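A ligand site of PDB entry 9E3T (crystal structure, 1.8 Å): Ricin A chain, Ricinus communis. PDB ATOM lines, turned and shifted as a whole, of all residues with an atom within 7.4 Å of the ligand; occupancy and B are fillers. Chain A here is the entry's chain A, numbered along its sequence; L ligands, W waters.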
ATOM      1  N   TYR A 187     -33.947 -17.929  18.575  1.00  0.00           N
ATOM      2  CA  TYR A 187     -33.457 -19.139  17.939  1.00  0.00           C
ATOM      3  C   TYR A 187     -34.550 -20.198  17.872  1.00  0.00           C
ATOM      4  O   TYR A 187     -34.751 -20.842  16.834  1.00  0.00           O
ATOM      5  CB  TYR A 187     -32.233 -19.666  18.690  1.00  0.00           C
ATOM      6  CG  TYR A 187     -31.625 -20.920  18.102  1.00  0.00           C
ATOM      7  CD1 TYR A 187     -30.733 -20.849  17.045  1.00  0.00           C
ATOM      8  CD2 TYR A 187     -31.940 -22.171  18.616  1.00  0.00           C
ATOM      9  CE1 TYR A 187     -30.166 -22.000  16.514  1.00  0.00           C
ATOM     10  CE2 TYR A 187     -31.388 -23.320  18.094  1.00  0.00           C
ATOM     11  CZ  TYR A 187     -30.499 -23.227  17.039  1.00  0.00           C
ATOM     12  OH  TYR A 187     -29.938 -24.371  16.518  1.00  0.00           O
ATOM     13  N   GLU A 191     -36.718 -21.949  14.888  1.00  0.00           N
ATOM     14  CA  GLU A 191     -36.908 -23.390  14.748  1.00  0.00           C
ATOM     15  C   GLU A 191     -38.354 -23.737  14.428  1.00  0.00           C
ATOM     16  O   GLU A 191     -38.618 -24.660  13.638  1.00  0.00           O
ATOM     17  CB  GLU A 191     -36.459 -24.105  16.030  1.00  0.00           C
ATOM     18  CG  GLU A 191     -34.961 -24.140  16.243  1.00  0.00           C
ATOM     19  CD  GLU A 191     -34.270 -25.221  15.419  1.00  0.00           C
ATOM     20  OE1 GLU A 191     -34.982 -26.067  14.835  1.00  0.00           O
ATOM     21  OE2 GLU A 191     -33.028 -25.223  15.368  1.00  0.00           O
ATOM     22  N   ASP A 205     -33.982 -30.520  18.403  1.00  0.00           N
ATOM     23  CA  ASP A 205     -32.646 -31.112  18.451  1.00  0.00           C
ATOM     24  C   ASP A 205     -31.896 -30.616  19.678  1.00  0.00           C
ATOM     25  O   ASP A 205     -32.380 -29.754  20.409  1.00  0.00           O
ATOM     26  CB  ASP A 205     -31.926 -30.820  17.118  1.00  0.00           C
ATOM     27  CG  ASP A 205     -31.590 -29.352  16.922  1.00  0.00           C
ATOM     28  OD1 ASP A 205     -31.584 -28.558  17.885  1.00  0.00           O
ATOM     29  OD2 ASP A 205     -31.301 -28.980  15.757  1.00  0.00           O
ATOM     30  N   PRO A 206     -30.709 -31.173  19.968  1.00  0.00           N
ATOM     31  CA  PRO A 206     -30.050 -30.847  21.249  1.00  0.00           C
ATOM     32  C   PRO A 206     -29.730 -29.382  21.455  1.00  0.00           C
ATOM     33  O   PRO A 206     -29.618 -28.947  22.613  1.00  0.00           O
ATOM     34  CB  PRO A 206     -28.770 -31.701  21.213  1.00  0.00           C
ATOM     35  CG  PRO A 206     -29.081 -32.820  20.317  1.00  0.00           C
ATOM     36  CD  PRO A 206     -29.985 -32.261  19.267  1.00  0.00           C
ATOM     37  N   SER A 207     -29.545 -28.604  20.393  1.00  0.00           N
ATOM     38  CA  SER A 207     -29.280 -27.174  20.560  1.00  0.00           C
ATOM     39  C   SER A 207     -30.476 -26.468  21.184  1.00  0.00           C
ATOM     40  O   SER A 207     -30.314 -25.565  22.013  1.00  0.00           O
ATOM     41  CB  SER A 207     -28.916 -26.541  19.218  1.00  0.00           C
ATOM     42  OG  SER A 207     -30.035 -26.492  18.356  1.00  0.00           O
ATOM     43  N   VAL A 208     -31.677 -26.877  20.801  1.00  0.00           N
ATOM     44  CA  VAL A 208     -32.890 -26.276  21.353  1.00  0.00           C
ATOM     45  C   VAL A 208     -33.065 -26.692  22.807  1.00  0.00           C
ATOM     46  O   VAL A 208     -33.348 -25.858  23.676  1.00  0.00           O
ATOM     47  CB  VAL A 208     -34.113 -26.681  20.503  1.00  0.00           C
ATOM     48  CG1 VAL A 208     -35.410 -26.199  21.165  1.00  0.00           C
ATOM     49  CG2 VAL A 208     -33.972 -26.134  19.100  1.00  0.00           C
ATOM     50  N   THR A 210     -30.938 -27.713  25.079  1.00  0.00           N
ATOM     51  CA  THR A 210     -29.968 -27.143  26.002  1.00  0.00           C
ATOM     52  C   THR A 210     -30.200 -25.648  26.208  1.00  0.00           C
ATOM     53  O   THR A 210     -29.997 -25.138  27.323  1.00  0.00           O
ATOM     54  CB  THR A 210     -28.550 -27.431  25.515  1.00  0.00           C
ATOM     55  OG1 THR A 210     -28.227 -28.801  25.785  1.00  0.00           O
ATOM     56  CG2 THR A 210     -27.511 -26.541  26.205  1.00  0.00           C
ATOM     57  N   LEU A 211     -30.628 -24.917  25.173  1.00  0.00           N
ATOM     58  CA  LEU A 211     -30.997 -23.525  25.375  1.00  0.00           C
ATOM     59  C   LEU A 211     -32.155 -23.409  26.355  1.00  0.00           C
ATOM     60  O   LEU A 211     -32.131 -22.553  27.256  1.00  0.00           O
ATOM     61  CB  LEU A 211     -31.358 -22.858  24.046  1.00  0.00           C
ATOM     62  CG  LEU A 211     -30.279 -22.286  23.151  1.00  0.00           C
ATOM     63  CD1 LEU A 211     -30.941 -21.713  21.894  1.00  0.00           C
ATOM     64  CD2 LEU A 211     -29.467 -21.198  23.850  1.00  0.00           C
ATOM     65  N   LEU A 218     -28.388 -18.499  31.788  1.00  0.00           N
ATOM     66  CA  LEU A 218     -27.992 -17.465  30.845  1.00  0.00           C
ATOM     67  C   LEU A 218     -28.427 -16.080  31.333  1.00  0.00           C
ATOM     68  O   LEU A 218     -27.664 -15.112  31.196  1.00  0.00           O
ATOM     69  CB  LEU A 218     -28.568 -17.743  29.456  1.00  0.00           C
ATOM     70  CG  LEU A 218     -28.006 -18.936  28.688  1.00  0.00           C
ATOM     71  CD1 LEU A 218     -28.882 -19.264  27.486  1.00  0.00           C
ATOM     72  CD2 LEU A 218     -26.579 -18.679  28.248  1.00  0.00           C
ATOM     73  N   LEU A 236     -22.964 -24.870  25.978  1.00  0.00           N
ATOM     74  CA  LEU A 236     -24.161 -25.092  25.191  1.00  0.00           C
ATOM     75  C   LEU A 236     -23.906 -26.265  24.233  1.00  0.00           C
ATOM     76  O   LEU A 236     -22.813 -26.835  24.199  1.00  0.00           O
ATOM     77  CB  LEU A 236     -24.557 -23.835  24.426  1.00  0.00           C
ATOM     78  CG  LEU A 236     -25.009 -22.644  25.265  1.00  0.00           C
ATOM     79  CD1 LEU A 236     -25.346 -21.463  24.377  1.00  0.00           C
ATOM     80  CD2 LEU A 236     -26.211 -23.020  26.128  1.00  0.00           C
ATOM     81  N   GLN A 237     -24.931 -26.626  23.468  1.00  0.00           N
ATOM     82  CA  GLN A 237     -24.871 -27.750  22.547  1.00  0.00           C
ATOM     83  C   GLN A 237     -25.093 -27.286  21.109  1.00  0.00           C
ATOM     84  O   GLN A 237     -25.909 -26.401  20.850  1.00  0.00           O
ATOM     85  CB  GLN A 237     -25.923 -28.811  22.888  1.00  0.00           C
ATOM     86  CG  GLN A 237     -25.394 -29.969  23.696  1.00  0.00           C
ATOM     87  CD  GLN A 237     -26.405 -31.068  23.875  1.00  0.00           C
ATOM     88  OE1 GLN A 237     -27.543 -30.820  24.285  1.00  0.00           O
ATOM     89  NE2 GLN A 237     -26.008 -32.294  23.572  1.00  0.00           N
ATOM     90  N   ARG A 238     -24.346 -27.894  20.189  1.00  0.00           N
ATOM     91  CA  ARG A 238     -24.580 -27.727  18.759  1.00  0.00           C
ATOM     92  C   ARG A 238     -25.742 -28.625  18.328  1.00  0.00           C
ATOM     93  O   ARG A 238     -26.271 -29.417  19.112  1.00  0.00           O
ATOM     94  CB  ARG A 238     -23.314 -28.055  17.969  1.00  0.00           C
ATOM     95  CG  ARG A 238     -22.105 -27.221  18.378  1.00  0.00           C
ATOM     96  CD  ARG A 238     -20.994 -27.306  17.336  1.00  0.00           C
ATOM     97  NE  ARG A 238     -19.879 -26.424  17.679  1.00  0.00           N
ATOM     98  CZ  ARG A 238     -19.850 -25.122  17.446  1.00  0.00           C
ATOM     99  NH1 ARG A 238     -20.849 -24.510  16.827  1.00  0.00           N
ATOM    100  NH2 ARG A 238     -18.797 -24.414  17.836  1.00  0.00           N
ATOM    101  N   ARG A 239     -26.144 -28.516  17.058  1.00  0.00           N
ATOM    102  CA  ARG A 239     -27.212 -29.373  16.549  1.00  0.00           C
ATOM    103  C   ARG A 239     -26.818 -30.841  16.564  1.00  0.00           C
ATOM    104  O   ARG A 239     -27.673 -31.716  16.732  1.00  0.00           O
ATOM    105  CB  ARG A 239     -27.626 -28.954  15.139  1.00  0.00           C
ATOM    106  CG  ARG A 239     -28.263 -27.571  15.031  1.00  0.00           C
ATOM    107  CD  ARG A 239     -28.793 -27.325  13.621  1.00  0.00           C
ATOM    108  NE  ARG A 239     -29.215 -25.951  13.421  1.00  0.00           N
ATOM    109  CZ  ARG A 239     -30.435 -25.498  13.663  1.00  0.00           C
ATOM    110  NH1 ARG A 239     -31.387 -26.281  14.124  1.00  0.00           N
ATOM    111  NH2 ARG A 239     -30.707 -24.216  13.428  1.00  0.00           N
ATOM    112  N   ASN A 240     -25.534 -31.146  16.375  1.00  0.00           N
ATOM    113  CA  ASN A 240     -25.065 -32.529  16.396  1.00  0.00           C
ATOM    114  C   ASN A 240     -24.731 -33.024  17.791  1.00  0.00           C
ATOM    115  O   ASN A 240     -24.147 -34.096  17.937  1.00  0.00           O
ATOM    116  CB  ASN A 240     -23.842 -32.700  15.467  1.00  0.00           C
ATOM    117  CG  ASN A 240     -22.601 -31.956  15.960  1.00  0.00           C
ATOM    118  OD1 ASN A 240     -22.541 -31.470  17.088  1.00  0.00           O
ATOM    119  ND2 ASN A 240     -21.586 -31.884  15.097  1.00  0.00           N
ATOM    120  N   GLY A 241     -25.061 -32.253  18.830  1.00  0.00           N
ATOM    121  CA  GLY A 241     -24.877 -32.679  20.197  1.00  0.00           C
ATOM    122  C   GLY A 241     -23.535 -32.341  20.819  1.00  0.00           C
ATOM    123  O   GLY A 241     -23.372 -32.547  22.025  1.00  0.00           O
ATOM    124  N   SER A 242     -22.578 -31.855  20.044  1.00  0.00           N
ATOM    125  CA  SER A 242     -21.289 -31.514  20.611  1.00  0.00           C
ATOM    126  C   SER A 242     -21.392 -30.248  21.452  1.00  0.00           C
ATOM    127  O   SER A 242     -22.293 -29.422  21.279  1.00  0.00           O
ATOM    128  CB  SER A 242     -20.242 -31.339  19.509  1.00  0.00           C
ATOM    129  OG  SER A 242     -20.636 -30.338  18.586  1.00  0.00           O
ATOM    130  N   PHE A 244     -19.862 -26.662  23.213  1.00  0.00           N
ATOM    131  CA  PHE A 244     -18.960 -25.516  23.068  1.00  0.00           C
ATOM    132  C   PHE A 244     -19.229 -24.527  24.187  1.00  0.00           C
ATOM    133  O   PHE A 244     -20.302 -24.519  24.790  1.00  0.00           O
ATOM    134  CB  PHE A 244     -19.107 -24.849  21.690  1.00  0.00           C
ATOM    135  CG  PHE A 244     -20.393 -24.098  21.512  1.00  0.00           C
ATOM    136  CD1 PHE A 244     -21.570 -24.773  21.235  1.00  0.00           C
ATOM    137  CD2 PHE A 244     -20.421 -22.715  21.595  1.00  0.00           C
ATOM    138  CE1 PHE A 244     -22.755 -24.087  21.070  1.00  0.00           C
ATOM    139  CE2 PHE A 244     -21.610 -22.020  21.420  1.00  0.00           C
ATOM    140  CZ  PHE A 244     -22.779 -22.713  21.162  1.00  0.00           C
ATOM    141  N   VAL A 246     -19.425 -20.642  25.841  1.00  0.00           N
ATOM    142  CA  VAL A 246     -19.761 -19.245  25.612  1.00  0.00           C
ATOM    143  C   VAL A 246     -19.137 -18.420  26.730  1.00  0.00           C
ATOM    144  O   VAL A 246     -19.340 -18.724  27.911  1.00  0.00           O
ATOM    145  CB  VAL A 246     -21.274 -19.023  25.549  1.00  0.00           C
ATOM    146  CG1 VAL A 246     -21.591 -17.535  25.432  1.00  0.00           C
ATOM    147  CG2 VAL A 246     -21.885 -19.801  24.386  1.00  0.00           C
ATOM    148  N   ILE A 251     -22.290 -13.180  21.530  1.00  0.00           N
ATOM    149  CA  ILE A 251     -22.784 -14.254  20.681  1.00  0.00           C
ATOM    150  C   ILE A 251     -24.253 -14.579  20.917  1.00  0.00           C
ATOM    151  O   ILE A 251     -24.901 -15.215  20.069  1.00  0.00           O
ATOM    152  CB  ILE A 251     -21.911 -15.521  20.875  1.00  0.00           C
ATOM    153  CG1 ILE A 251     -21.949 -16.421  19.655  1.00  0.00           C
ATOM    154  CG2 ILE A 251     -22.371 -16.307  22.091  1.00  0.00           C
ATOM    155  CD1 ILE A 251     -21.028 -17.616  19.781  1.00  0.00           C
ATOM    156  N   LEU A 252     -24.808 -14.153  22.060  1.00  0.00           N
ATOM    157  CA  LEU A 252     -26.158 -14.537  22.463  1.00  0.00           C
ATOM    158  C   LEU A 252     -27.222 -13.523  22.092  1.00  0.00           C
ATOM    159  O   LEU A 252     -28.409 -13.845  22.154  1.00  0.00           O
ATOM    160  CB  LEU A 252     -26.190 -14.764  23.982  1.00  0.00           C
ATOM    161  CG  LEU A 252     -25.322 -15.892  24.523  1.00  0.00           C
ATOM    162  CD1 LEU A 252     -25.175 -15.783  26.034  1.00  0.00           C
ATOM    163  CD2 LEU A 252     -25.906 -17.236  24.122  1.00  0.00           C
ATOM    164  N   ILE A 253     -26.830 -12.310  21.703  1.00  0.00           N
ATOM    165  CA  ILE A 253     -27.779 -11.235  21.421  1.00  0.00           C
ATOM    166  C   ILE A 253     -28.797 -11.640  20.359  1.00  0.00           C
ATOM    167  O   ILE A 253     -29.993 -11.372  20.533  1.00  0.00           O
ATOM    168  CB  ILE A 253     -27.044  -9.939  21.034  1.00  0.00           C
ATOM    169  CG1 ILE A 253     -26.227  -9.445  22.226  1.00  0.00           C
ATOM    170  CG2 ILE A 253     -28.026  -8.879  20.575  1.00  0.00           C
ATOM    171  CD1 ILE A 253     -25.552  -8.099  22.010  1.00  0.00           C
ATOM    172  N   PRO A 254     -28.418 -12.304  19.255  1.00  0.00           N
ATOM    173  CA  PRO A 254     -29.429 -12.744  18.291  1.00  0.00           C
ATOM    174  C   PRO A 254     -30.193 -13.989  18.721  1.00  0.00           C
ATOM    175  O   PRO A 254     -31.130 -14.391  18.022  1.00  0.00           O
ATOM    176  CB  PRO A 254     -28.615 -13.016  17.019  1.00  0.00           C
ATOM    177  CG  PRO A 254     -27.243 -12.525  17.286  1.00  0.00           C
ATOM    178  CD  PRO A 254     -27.057 -12.593  18.752  1.00  0.00           C
ATOM    179  N   ILE A 255     -29.826 -14.596  19.845  1.00  0.00           N
ATOM    180  CA  ILE A 255     -30.312 -15.919  20.223  1.00  0.00           C
ATOM    181  C   ILE A 255     -31.365 -15.846  21.320  1.00  0.00           C
ATOM    182  O   ILE A 255     -32.394 -16.527  21.259  1.00  0.00           O
ATOM    183  CB  ILE A 255     -29.128 -16.820  20.658  1.00  0.00           C
ATOM    184  CG1 ILE A 255     -28.129 -16.963  19.508  1.00  0.00           C
ATOM    185  CG2 ILE A 255     -29.630 -18.171  21.164  1.00  0.00           C
ATOM    186  CD1 ILE A 255     -28.729 -17.550  18.246  1.00  0.00           C
ATOM    187  N   ILE A 256     -31.124 -15.043  22.358  1.00  0.00           N
ATOM    188  CA  ILE A 256     -32.042 -14.906  23.475  1.00  0.00           C
ATOM    189  C   ILE A 256     -32.776 -13.575  23.362  1.00  0.00           C
ATOM    190  O   ILE A 256     -32.173 -12.548  23.014  1.00  0.00           O
ATOM    191  CB  ILE A 256     -31.295 -15.041  24.817  1.00  0.00           C
ATOM    192  CG1 ILE A 256     -32.283 -14.976  25.990  1.00  0.00           C
ATOM    193  CG2 ILE A 256     -30.197 -14.005  24.943  1.00  0.00           C
ATOM    194  CD1 ILE A 256     -31.697 -15.434  27.323  1.00  0.00           C
HETATM  195  C1  LIG L   1     -25.595 -22.415  18.049  1.00  0.00           C
HETATM  196  C2  LIG L   1     -25.115 -24.488  16.604  1.00  0.00           C
HETATM  197  C3  LIG L   1     -24.499 -25.632  15.826  1.00  0.00           C
HETATM  198  C4  LIG L   1     -27.777 -22.782  20.686  1.00  0.00           C
HETATM  199  C5  LIG L   1     -26.272 -22.629  20.839  1.00  0.00           C
HETATM  200  C6  LIG L   1     -25.813 -21.293  20.288  1.00  0.00           C
HETATM  201  C7  LIG L   1     -25.725 -20.189  21.130  1.00  0.00           C
HETATM  202  C8  LIG L   1     -25.307 -18.965  20.614  1.00  0.00           C
HETATM  203  C9  LIG L   1     -24.987 -18.854  19.273  1.00  0.00           C
HETATM  204  C10 LIG L   1     -25.075 -19.960  18.440  1.00  0.00           C
HETATM  205  C11 LIG L   1     -24.716 -19.818  16.964  1.00  0.00           C
HETATM  206  C12 LIG L   1     -25.498 -21.174  18.947  1.00  0.00           C
HETATM  207  C13 LIG L   1     -26.751 -23.030  17.548  1.00  0.00           C
HETATM  208  C14 LIG L   1     -26.476 -24.184  16.755  1.00  0.00           C
HETATM  209  O1  LIG L   1     -23.248 -25.711  15.738  1.00  0.00           O
HETATM  210  O2  LIG L   1     -25.221 -26.485  15.261  1.00  0.00           O
HETATM  211  S1  LIG L   1     -24.284 -23.311  17.486  1.00  0.00           S
HETATM  212  O   HOH W   1     -27.652 -25.177  22.850  1.00  0.00           O
HETATM  213  O   HOH W   2     -23.851 -29.603  14.480  1.00  0.00           O
HETATM  214  O   HOH W   3     -25.004 -26.754  12.708  1.00  0.00           O
HETATM  215  O   HOH W   4     -27.080 -24.707  12.954  1.00  0.00           O
HETATM  216  O   HOH W   5     -22.597 -26.948  13.378  1.00  0.00           O
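The backbone NH (N) of Arg 239 is in hydrogen-bond range of an oxygen (O2) of the ligand (2.9 Å).
The guanidinium group (NH1) of Arg 238 is in salt-bridge range of an oxygen (O1) of the ligand (2.9 Å).
OH of Tyr 187 touches C14 of the ligand, at 3.5 Å.
O of Ser 207 touches C4 of the ligand, 3.99 Å away.
Leu 211 touches the ligand (CG to C4, 3.5 Å).
Leu 236 touches the ligand (CD1 to C7, 3.5 Å).
O of Gln 237 touches C5 of the ligand (3.8 Å).
Phe 244 touches the ligand.
Ile 251 touches the ligand (O to C9, 3.7 Å).
CD2 of Leu 252 touches C8 of the ligand, at 3.96 Å.
Ile 255 touches the ligand (CG1 to C8, 3.6 Å).
Within 4 Å of the ligand: Tyr 187, Ser 207, Leu 211, Leu 236, Gln 237, Arg 238, Arg 239, Phe 244, Ile 251, Leu 252 and Ile 255.
Along chain A the residues within 4 Å of the ligand span positions 187 to 255.
Water W1 bridges O of Ser 207 (2.8 Å) and O of Gln 237 (2.9 Å).
Water W4 bridges the guanidinium group of Arg 239 (2.5 Å) and an oxygen (O2) of the ligand (3.5 Å).
Water W2 lies within hydrogen-bond range of the backbone NH of Asn 240 and an oxygen (O2) of the ligand.
The guanidinium group of Arg 239 lies within salt-bridge range of the side-chain carboxylate of Asp 205, at 3.2 Å.
NH2 of Arg 239 lies within salt-bridge range of OE2 of Glu 191.
The backbone carbonyl oxygen (O) of Ile 255 lies within hydrogen-bond range of the backbone NH (N) of Tyr 187.
The side-chain hydroxyl of Tyr 187 sits at hydrogen-bond distance from the side-chain hydroxyl of Ser 207, at 2.8 Å.
OE1 of Gln 237 lies within hydrogen-bond range of OG1 of Thr 210 (2.6 Å).
OE1 of Gln 237 lies close to O of Pro 206.
NE2 of Gln 237 sits at hydrogen-bond distance from O of Gly 241 (3.1 Å).
The side-chain hydroxyl (OG) of Ser 207 is in hydrogen-bond range of the side-chain carboxylate (OD1) of Asp 205 (2.6 Å).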
